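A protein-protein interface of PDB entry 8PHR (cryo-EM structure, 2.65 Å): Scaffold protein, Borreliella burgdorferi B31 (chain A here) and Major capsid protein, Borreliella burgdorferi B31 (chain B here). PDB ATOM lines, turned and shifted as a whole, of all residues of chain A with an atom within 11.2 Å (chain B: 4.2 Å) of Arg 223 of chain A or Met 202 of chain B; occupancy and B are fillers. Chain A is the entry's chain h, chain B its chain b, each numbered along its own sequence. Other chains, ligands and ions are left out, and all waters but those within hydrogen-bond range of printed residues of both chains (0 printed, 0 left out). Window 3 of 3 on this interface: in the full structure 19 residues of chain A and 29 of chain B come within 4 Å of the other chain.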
ATOM      1  N   ARG A 214     -15.279   1.503   8.185  1.00  0.00           N
ATOM      2  CA  ARG A 214     -15.365   0.246   8.926  1.00  0.00           C
ATOM      3  C   ARG A 214     -14.143  -0.629   8.672  1.00  0.00           C
ATOM      4  O   ARG A 214     -13.586  -1.227   9.604  1.00  0.00           O
ATOM      5  CB  ARG A 214     -16.645  -0.501   8.552  1.00  0.00           C
ATOM      6  CG  ARG A 214     -16.745  -1.893   9.160  1.00  0.00           C
ATOM      7  CD  ARG A 214     -17.607  -2.810   8.309  1.00  0.00           C
ATOM      8  NE  ARG A 214     -18.864  -2.178   7.932  1.00  0.00           N
ATOM      9  CZ  ARG A 214     -19.709  -2.668   7.035  1.00  0.00           C
ATOM     10  NH1 ARG A 214     -19.460  -3.800   6.397  1.00  0.00           N
ATOM     11  NH2 ARG A 214     -20.832  -2.006   6.772  1.00  0.00           N
ATOM     12  N   PHE A 217     -11.213   0.821  10.549  1.00  0.00           N
ATOM     13  CA  PHE A 217     -11.327   0.573  11.982  1.00  0.00           C
ATOM     14  C   PHE A 217     -10.947  -0.862  12.316  1.00  0.00           C
ATOM     15  O   PHE A 217     -10.254  -1.112  13.309  1.00  0.00           O
ATOM     16  CB  PHE A 217     -12.746   0.879  12.466  1.00  0.00           C
ATOM     17  CG  PHE A 217     -13.040   0.355  13.845  1.00  0.00           C
ATOM     18  CD1 PHE A 217     -12.643   1.066  14.965  1.00  0.00           C
ATOM     19  CD2 PHE A 217     -13.709  -0.847  14.023  1.00  0.00           C
ATOM     20  CE1 PHE A 217     -12.907   0.592  16.235  1.00  0.00           C
ATOM     21  CE2 PHE A 217     -13.971  -1.326  15.292  1.00  0.00           C
ATOM     22  CZ  PHE A 217     -13.573  -0.605  16.399  1.00  0.00           C
ATOM     23  N   TYR A 218     -11.392  -1.821  11.500  1.00  0.00           N
ATOM     24  CA  TYR A 218     -11.012  -3.208  11.749  1.00  0.00           C
ATOM     25  C   TYR A 218      -9.526  -3.441  11.498  1.00  0.00           C
ATOM     26  O   TYR A 218      -8.910  -4.275  12.172  1.00  0.00           O
ATOM     27  CB  TYR A 218     -11.857  -4.153  10.896  1.00  0.00           C
ATOM     28  CG  TYR A 218     -13.201  -4.466  11.512  1.00  0.00           C
ATOM     29  CD1 TYR A 218     -13.291  -4.944  12.813  1.00  0.00           C
ATOM     30  CD2 TYR A 218     -14.377  -4.286  10.798  1.00  0.00           C
ATOM     31  CE1 TYR A 218     -14.512  -5.232  13.388  1.00  0.00           C
ATOM     32  CE2 TYR A 218     -15.607  -4.571  11.365  1.00  0.00           C
ATOM     33  CZ  TYR A 218     -15.667  -5.045  12.659  1.00  0.00           C
ATOM     34  OH  TYR A 218     -16.885  -5.332  13.231  1.00  0.00           O
ATOM     35  N   GLU A 219      -8.937  -2.723  10.539  1.00  0.00           N
ATOM     36  CA  GLU A 219      -7.499  -2.829  10.310  1.00  0.00           C
ATOM     37  C   GLU A 219      -6.707  -2.303  11.502  1.00  0.00           C
ATOM     38  O   GLU A 219      -5.711  -2.913  11.911  1.00  0.00           O
ATOM     39  CB  GLU A 219      -7.113  -2.076   9.038  1.00  0.00           C
ATOM     40  CG  GLU A 219      -7.522  -2.769   7.749  1.00  0.00           C
ATOM     41  CD  GLU A 219      -7.230  -1.929   6.520  1.00  0.00           C
ATOM     42  OE1 GLU A 219      -6.722  -0.799   6.677  1.00  0.00           O
ATOM     43  OE2 GLU A 219      -7.506  -2.399   5.397  1.00  0.00           O
ATOM     44  N   ASN A 220      -7.131  -1.176  12.068  1.00  0.00           N
ATOM     45  CA  ASN A 220      -6.419  -0.546  13.173  1.00  0.00           C
ATOM     46  C   ASN A 220      -6.832  -1.083  14.539  1.00  0.00           C
ATOM     47  O   ASN A 220      -6.249  -0.674  15.548  1.00  0.00           O
ATOM     48  CB  ASN A 220      -6.629   0.972  13.136  1.00  0.00           C
ATOM     49  CG  ASN A 220      -6.154   1.595  11.838  1.00  0.00           C
ATOM     50  OD1 ASN A 220      -5.611   0.912  10.970  1.00  0.00           O
ATOM     51  ND2 ASN A 220      -6.358   2.900  11.699  1.00  0.00           N
ATOM     52  N   LEU A 221      -7.815  -1.977  14.597  1.00  0.00           N
ATOM     53  CA  LEU A 221      -8.277  -2.505  15.874  1.00  0.00           C
ATOM     54  C   LEU A 221      -7.209  -3.386  16.513  1.00  0.00           C
ATOM     55  O   LEU A 221      -6.575  -4.202  15.838  1.00  0.00           O
ATOM     56  CB  LEU A 221      -9.569  -3.298  15.681  1.00  0.00           C
ATOM     57  CG  LEU A 221     -10.116  -4.037  16.903  1.00  0.00           C
ATOM     58  CD1 LEU A 221     -10.572  -3.053  17.971  1.00  0.00           C
ATOM     59  CD2 LEU A 221     -11.251  -4.968  16.505  1.00  0.00           C
ATOM     60  N   LYS A 222      -7.012  -3.216  17.819  1.00  0.00           N
ATOM     61  CA  LYS A 222      -6.077  -4.026  18.598  1.00  0.00           C
ATOM     62  C   LYS A 222      -6.767  -4.410  19.904  1.00  0.00           C
ATOM     63  O   LYS A 222      -6.747  -3.646  20.874  1.00  0.00           O
ATOM     64  CB  LYS A 222      -4.774  -3.273  18.851  1.00  0.00           C
ATOM     65  CG  LYS A 222      -4.938  -1.767  18.960  1.00  0.00           C
ATOM     66  CD  LYS A 222      -3.594  -1.071  19.091  1.00  0.00           C
ATOM     67  CE  LYS A 222      -3.760   0.438  19.172  1.00  0.00           C
ATOM     68  NZ  LYS A 222      -2.454   1.136  19.327  1.00  0.00           N
ATOM     69  N   ARG A 223      -7.375  -5.592  19.924  1.00  0.00           N
ATOM     70  CA  ARG A 223      -8.101  -6.061  21.094  1.00  0.00           C
ATOM     71  C   ARG A 223      -7.140  -6.508  22.190  1.00  0.00           C
ATOM     72  O   ARG A 223      -6.022  -6.957  21.922  1.00  0.00           O
ATOM     73  CB  ARG A 223      -9.030  -7.217  20.719  1.00  0.00           C
ATOM     74  CG  ARG A 223     -10.114  -6.857  19.715  1.00  0.00           C
ATOM     75  CD  ARG A 223     -10.873  -8.100  19.258  1.00  0.00           C
ATOM     76  NE  ARG A 223     -12.011  -7.788  18.399  1.00  0.00           N
ATOM     77  CZ  ARG A 223     -13.092  -7.121  18.782  1.00  0.00           C
ATOM     78  NH1 ARG A 223     -13.253  -6.718  20.033  1.00  0.00           N
ATOM     79  NH2 ARG A 223     -14.045  -6.865  17.890  1.00  0.00           N
ATOM     80  N   HIS A 224      -7.589  -6.375  23.436  1.00  0.00           N
ATOM     81  CA  HIS A 224      -6.833  -6.870  24.580  1.00  0.00           C
ATOM     82  C   HIS A 224      -7.170  -8.340  24.796  1.00  0.00           C
ATOM     83  O   HIS A 224      -8.339  -8.693  24.988  1.00  0.00           O
ATOM     84  CB  HIS A 224      -7.153  -6.046  25.826  1.00  0.00           C
ATOM     85  CG  HIS A 224      -6.337  -6.415  27.026  1.00  0.00           C
ATOM     86  ND1 HIS A 224      -4.963  -6.314  27.052  1.00  0.00           N
ATOM     87  CD2 HIS A 224      -6.702  -6.881  28.244  1.00  0.00           C
ATOM     88  CE1 HIS A 224      -4.516  -6.703  28.233  1.00  0.00           C
ATOM     89  NE2 HIS A 224      -5.552  -7.052  28.975  1.00  0.00           N
ATOM     90  N   LYS A 225      -6.151  -9.197  24.768  1.00  0.00           N
ATOM     91  CA  LYS A 225      -6.347 -10.639  24.825  1.00  0.00           C
ATOM     92  C   LYS A 225      -6.204 -11.212  26.228  1.00  0.00           C
ATOM     93  O   LYS A 225      -6.281 -12.433  26.393  1.00  0.00           O
ATOM     94  CB  LYS A 225      -5.367 -11.339  23.875  1.00  0.00           C
ATOM     95  CG  LYS A 225      -5.530 -10.927  22.420  1.00  0.00           C
ATOM     96  CD  LYS A 225      -4.602 -11.708  21.504  1.00  0.00           C
ATOM     97  CE  LYS A 225      -4.834 -11.336  20.048  1.00  0.00           C
ATOM     98  NZ  LYS A 225      -4.008 -12.159  19.123  1.00  0.00           N
ATOM     99  N   ARG A 226      -6.001 -10.371  27.237  1.00  0.00           N
ATOM    100  CA  ARG A 226      -5.932 -10.839  28.617  1.00  0.00           C
ATOM    101  C   ARG A 226      -7.092 -10.286  29.440  1.00  0.00           C
ATOM    102  O   ARG A 226      -7.294 -10.681  30.588  1.00  0.00           O
ATOM    103  CB  ARG A 226      -4.600 -10.445  29.258  1.00  0.00           C
ATOM    104  CG  ARG A 226      -3.373 -10.907  28.490  1.00  0.00           C
ATOM    105  CD  ARG A 226      -2.100 -10.417  29.160  1.00  0.00           C
ATOM    106  NE  ARG A 226      -0.905 -10.788  28.411  1.00  0.00           N
ATOM    107  CZ  ARG A 226       0.330 -10.457  28.763  1.00  0.00           C
ATOM    108  NH1 ARG A 226       0.571  -9.746  29.853  1.00  0.00           N
ATOM    109  NH2 ARG A 226       1.349 -10.849  28.003  1.00  0.00           N
ATOM    110  N   TYR B  26     -19.175  -2.113  16.303  1.00  0.00           N
ATOM    111  CA  TYR B  26     -18.156  -2.818  15.533  1.00  0.00           C
ATOM    112  C   TYR B  26     -17.260  -3.665  16.428  1.00  0.00           C
ATOM    113  O   TYR B  26     -16.763  -4.711  15.995  1.00  0.00           O
ATOM    114  CB  TYR B  26     -17.316  -1.817  14.740  1.00  0.00           C
ATOM    115  CG  TYR B  26     -18.027  -1.195  13.559  1.00  0.00           C
ATOM    116  CD1 TYR B  26     -19.333  -1.546  13.242  1.00  0.00           C
ATOM    117  CD2 TYR B  26     -17.392  -0.248  12.767  1.00  0.00           C
ATOM    118  CE1 TYR B  26     -19.983  -0.975  12.164  1.00  0.00           C
ATOM    119  CE2 TYR B  26     -18.035   0.328  11.690  1.00  0.00           C
ATOM    120  CZ  TYR B  26     -19.329  -0.039  11.393  1.00  0.00           C
ATOM    121  OH  TYR B  26     -19.972   0.533  10.319  1.00  0.00           O
ATOM    122  N   LYS B  27     -17.040  -3.232  17.671  1.00  0.00           N
ATOM    123  CA  LYS B  27     -16.225  -4.001  18.604  1.00  0.00           C
ATOM    124  C   LYS B  27     -16.873  -5.325  18.985  1.00  0.00           C
ATOM    125  O   LYS B  27     -16.188  -6.206  19.517  1.00  0.00           O
ATOM    126  CB  LYS B  27     -15.958  -3.179  19.867  1.00  0.00           C
ATOM    127  CG  LYS B  27     -15.293  -1.838  19.612  1.00  0.00           C
ATOM    128  CD  LYS B  27     -15.388  -0.938  20.834  1.00  0.00           C
ATOM    129  CE  LYS B  27     -14.865  -1.636  22.079  1.00  0.00           C
ATOM    130  NZ  LYS B  27     -14.993  -0.779  23.290  1.00  0.00           N
ATOM    131  N   PHE B  29     -18.280  -7.511  16.898  1.00  0.00           N
ATOM    132  CA  PHE B  29     -18.266  -8.469  15.805  1.00  0.00           C
ATOM    133  C   PHE B  29     -16.885  -8.493  15.168  1.00  0.00           C
ATOM    134  O   PHE B  29     -16.102  -7.548  15.292  1.00  0.00           O
ATOM    135  CB  PHE B  29     -19.326  -8.133  14.744  1.00  0.00           C
ATOM    136  CG  PHE B  29     -20.734  -8.142  15.267  1.00  0.00           C
ATOM    137  CD1 PHE B  29     -21.349  -9.331  15.622  1.00  0.00           C
ATOM    138  CD2 PHE B  29     -21.443  -6.960  15.400  1.00  0.00           C
ATOM    139  CE1 PHE B  29     -22.645  -9.340  16.102  1.00  0.00           C
ATOM    140  CE2 PHE B  29     -22.739  -6.964  15.880  1.00  0.00           C
ATOM    141  CZ  PHE B  29     -23.341  -8.156  16.231  1.00  0.00           C
ATOM    142  N   MET B 201     -14.213 -16.163  21.387  1.00  0.00           N
ATOM    143  CA  MET B 201     -15.441 -15.908  22.126  1.00  0.00           C
ATOM    144  C   MET B 201     -15.487 -14.455  22.574  1.00  0.00           C
ATOM    145  O   MET B 201     -14.448 -13.820  22.785  1.00  0.00           O
ATOM    146  CB  MET B 201     -15.557 -16.832  23.343  1.00  0.00           C
ATOM    147  CG  MET B 201     -15.569 -18.310  22.997  1.00  0.00           C
ATOM    148  SD  MET B 201     -17.031 -18.807  22.070  1.00  0.00           S
ATOM    149  CE  MET B 201     -18.282 -18.734  23.349  1.00  0.00           C
ATOM    150  N   MET B 202     -16.703 -13.930  22.723  1.00  0.00           N
ATOM    151  CA  MET B 202     -16.919 -12.546  23.117  1.00  0.00           C
ATOM    152  C   MET B 202     -17.923 -12.504  24.259  1.00  0.00           C
ATOM    153  O   MET B 202     -18.978 -13.150  24.194  1.00  0.00           O
ATOM    154  CB  MET B 202     -17.421 -11.706  21.937  1.00  0.00           C
ATOM    155  CG  MET B 202     -17.908 -10.319  22.322  1.00  0.00           C
ATOM    156  SD  MET B 202     -16.589  -9.284  22.985  1.00  0.00           S
ATOM    157  CE  MET B 202     -15.680  -8.893  21.491  1.00  0.00           C
ATOM    158  N   VAL B 203     -17.585 -11.746  25.298  1.00  0.00           N
ATOM    159  CA  VAL B 203     -18.444 -11.529  26.454  1.00  0.00           C
ATOM    160  C   VAL B 203     -18.681 -10.032  26.587  1.00  0.00           C
ATOM    161  O   VAL B 203     -17.739  -9.238  26.479  1.00  0.00           O
ATOM    162  CB  VAL B 203     -17.825 -12.100  27.743  1.00  0.00           C
ATOM    163  CG1 VAL B 203     -18.828 -12.045  28.886  1.00  0.00           C
ATOM    164  CG2 VAL B 203     -17.341 -13.523  27.517  1.00  0.00           C
ATOM    165  N   TYR B 248     -12.486 -12.394  24.394  1.00  0.00           N
ATOM    166  CA  TYR B 248     -12.521 -10.957  24.605  1.00  0.00           C
ATOM    167  C   TYR B 248     -13.676 -10.582  25.525  1.00  0.00           C
ATOM    168  O   TYR B 248     -14.748 -11.193  25.490  1.00  0.00           O
ATOM    169  CB  TYR B 248     -12.648 -10.217  23.272  1.00  0.00           C
ATOM    170  CG  TYR B 248     -11.684 -10.704  22.213  1.00  0.00           C
ATOM    171  CD1 TYR B 248     -10.312 -10.656  22.422  1.00  0.00           C
ATOM    172  CD2 TYR B 248     -12.147 -11.215  21.008  1.00  0.00           C
ATOM    173  CE1 TYR B 248      -9.428 -11.100  21.459  1.00  0.00           C
ATOM    174  CE2 TYR B 248     -11.269 -11.664  20.039  1.00  0.00           C
ATOM    175  CZ  TYR B 248      -9.912 -11.603  20.270  1.00  0.00           C
ATOM    176  OH  TYR B 248      -9.034 -12.048  19.307  1.00  0.00           O
ATOM    177  N   GLU B 250     -15.830  -7.137  26.972  1.00  0.00           N
ATOM    178  CA  GLU B 250     -16.145  -5.735  26.754  1.00  0.00           C
ATOM    179  C   GLU B 250     -17.213  -5.294  27.744  1.00  0.00           C
ATOM    180  O   GLU B 250     -17.987  -6.103  28.266  1.00  0.00           O
ATOM    181  CB  GLU B 250     -16.628  -5.476  25.319  1.00  0.00           C
ATOM    182  CG  GLU B 250     -15.713  -6.022  24.235  1.00  0.00           C
ATOM    183  CD  GLU B 250     -14.336  -5.391  24.261  1.00  0.00           C
ATOM    184  OE1 GLU B 250     -14.250  -4.147  24.188  1.00  0.00           O
ATOM    185  OE2 GLU B 250     -13.339  -6.138  24.347  1.00  0.00           O
ATOM    186  N   LEU B 260     -23.613 -11.327  28.384  1.00  0.00           N
ATOM    187  CA  LEU B 260     -23.877 -11.900  27.069  1.00  0.00           C
ATOM    188  C   LEU B 260     -22.620 -12.595  26.569  1.00  0.00           C
ATOM    189  O   LEU B 260     -21.580 -11.951  26.412  1.00  0.00           O
ATOM    190  CB  LEU B 260     -24.315 -10.815  26.081  1.00  0.00           C
ATOM    191  CG  LEU B 260     -24.933 -11.278  24.762  1.00  0.00           C
ATOM    192  CD1 LEU B 260     -26.329 -11.820  24.993  1.00  0.00           C
ATOM    193  CD2 LEU B 260     -24.952 -10.138  23.758  1.00  0.00           C
ATOM    194  N   ILE B 261     -22.712 -13.896  26.308  1.00  0.00           N
ATOM    195  CA  ILE B 261     -21.581 -14.675  25.815  1.00  0.00           C
ATOM    196  C   ILE B 261     -21.958 -15.295  24.477  1.00  0.00           C
ATOM    197  O   ILE B 261     -23.008 -15.941  24.362  1.00  0.00           O
ATOM    198  CB  ILE B 261     -21.149 -15.759  26.820  1.00  0.00           C
ATOM    199  CG1 ILE B 261     -21.094 -15.180  28.237  1.00  0.00           C
ATOM    200  CG2 ILE B 261     -19.803 -16.347  26.426  1.00  0.00           C
ATOM    201  CD1 ILE B 261     -20.665 -16.175  29.289  1.00  0.00           C
ATOM    202  N   TYR B 262     -21.101 -15.102  23.472  1.00  0.00           N
ATOM    203  CA  TYR B 262     -21.380 -15.632  22.143  1.00  0.00           C
ATOM    204  C   TYR B 262     -20.077 -15.748  21.363  1.00  0.00           C
ATOM    205  O   TYR B 262     -19.143 -14.979  21.609  1.00  0.00           O
ATOM    206  CB  TYR B 262     -22.391 -14.745  21.395  1.00  0.00           C
ATOM    207  CG  TYR B 262     -21.941 -13.319  21.158  1.00  0.00           C
ATOM    208  CD1 TYR B 262     -21.120 -12.992  20.085  1.00  0.00           C
ATOM    209  CD2 TYR B 262     -22.342 -12.297  22.008  1.00  0.00           C
ATOM    210  CE1 TYR B 262     -20.711 -11.690  19.867  1.00  0.00           C
ATOM    211  CE2 TYR B 262     -21.938 -10.992  21.799  1.00  0.00           C
ATOM    212  CZ  TYR B 262     -21.123 -10.695  20.728  1.00  0.00           C
ATOM    213  OH  TYR B 262     -20.718  -9.396  20.515  1.00  0.00           O
ATOM    214  N   LEU B 264     -17.512 -15.607  17.947  1.00  0.00           N
ATOM    215  CA  LEU B 264     -17.250 -14.653  16.875  1.00  0.00           C
ATOM    216  C   LEU B 264     -17.053 -15.360  15.537  1.00  0.00           C
ATOM    217  O   LEU B 264     -16.209 -14.970  14.728  1.00  0.00           O
ATOM    218  CB  LEU B 264     -16.036 -13.789  17.203  1.00  0.00           C
ATOM    219  CG  LEU B 264     -16.169 -12.826  18.384  1.00  0.00           C
ATOM    220  CD1 LEU B 264     -15.005 -11.849  18.409  1.00  0.00           C
ATOM    221  CD2 LEU B 264     -17.492 -12.082  18.313  1.00  0.00           C
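The side-chain carboxylate of Glu 250 of chain B is in salt-bridge range of the side-chain amino group of Lys 27 of chain B (3.6 Å). The backbone NH of Met 202 of chain B is in hydrogen-bond range of the backbone carbonyl oxygen of Tyr 262 of chain B, 2.9 Å away. O of Met 201 of chain B is in hydrogen-bond range of N of Tyr 248 of chain B (2.9 Å). The backbone NH of Val 203 of chain B is in hydrogen-bond range of the backbone carbonyl oxygen of Tyr 248 of chain B (2.9 Å).
Hydrophobic or aromatic side chains of chain A that line the printed part of chain B: Phe 217 and Tyr 218. Hydrophobic or aromatic side chains of chain B that line the printed part of chain A: Tyr 26, Met 202 and Tyr 248. Along chain B the printed residues that touch a printed residue of chain A span positions 26 to 248. Among the printed residues, no Asp or Glu carboxylate lies within 4 Å of a Lys or Arg side-chain nitrogen of the other chain.
Arg 214 of chain A touches Tyr 26 of chain B. CE2 of Phe 217 of chain A touches CB of Tyr 26 of chain B, at 3.4 Å. Phe 217 of chain A touches Lys 27 of chain B. NH2 of Arg 223 of chain A touches O of Tyr 26 of chain B, at 3.95 Å. Arg 223 of chain A touches Met 202 of chain B. Arg 223 of chain A touches Tyr 248 of chain B (CD to CE2, 3.7 Å). Tyr 248 of chain B touches His 224 of chain A (CD1 to O, 3.8 Å).
Glu 219 of chain A touches none of the printed residues of chain B. Of chain B, only Tyr 26, Lys 27, Phe 29, Met 202 and Tyr 248 come within 4 Å of Arg 223 of chain A. Of the printed residues of chain B, His 224 of chain A touches Tyr 248 (3.8 Å). Of the printed residues of chain A, Tyr 26 of chain B touches Arg 214 (3.5 Å), Phe 217 (3.4 Å), Tyr 218 (2.8 Å) and Arg 223 (3.95 Å). Lys 27 of chain B touches just these residues of chain A: Phe 217 and Arg 223. Met 201 of chain B touches none of the printed residues of chain A. Met 202 of chain B touches one residue of chain A. No residue of chain A comes within 4 Å of Tyr 262 of chain B. The nearest residue of chain A that does not touch Met 202 of chain B is Leu 221 of chain A (7.7 Å).
O of Tyr 26 of chain B is in hydrogen-bond range of OH of Tyr 218 of chain A (2.8 Å). O of Lys 27 of chain B is in hydrogen-bond range of NH2 of Arg 223 of chain A, 2.8 Å away. The guanidinium group (NH2) of Arg 223 of chain A sits at hydrogen-bond distance from the backbone carbonyl oxygen (O) of Phe 29 of chain B. The side-chain hydroxyl (OH) of Tyr 218 of chain A sits at hydrogen-bond distance from the backbone carbonyl oxygen (O) of Phe 29 of chain B, 3.1 Å away.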
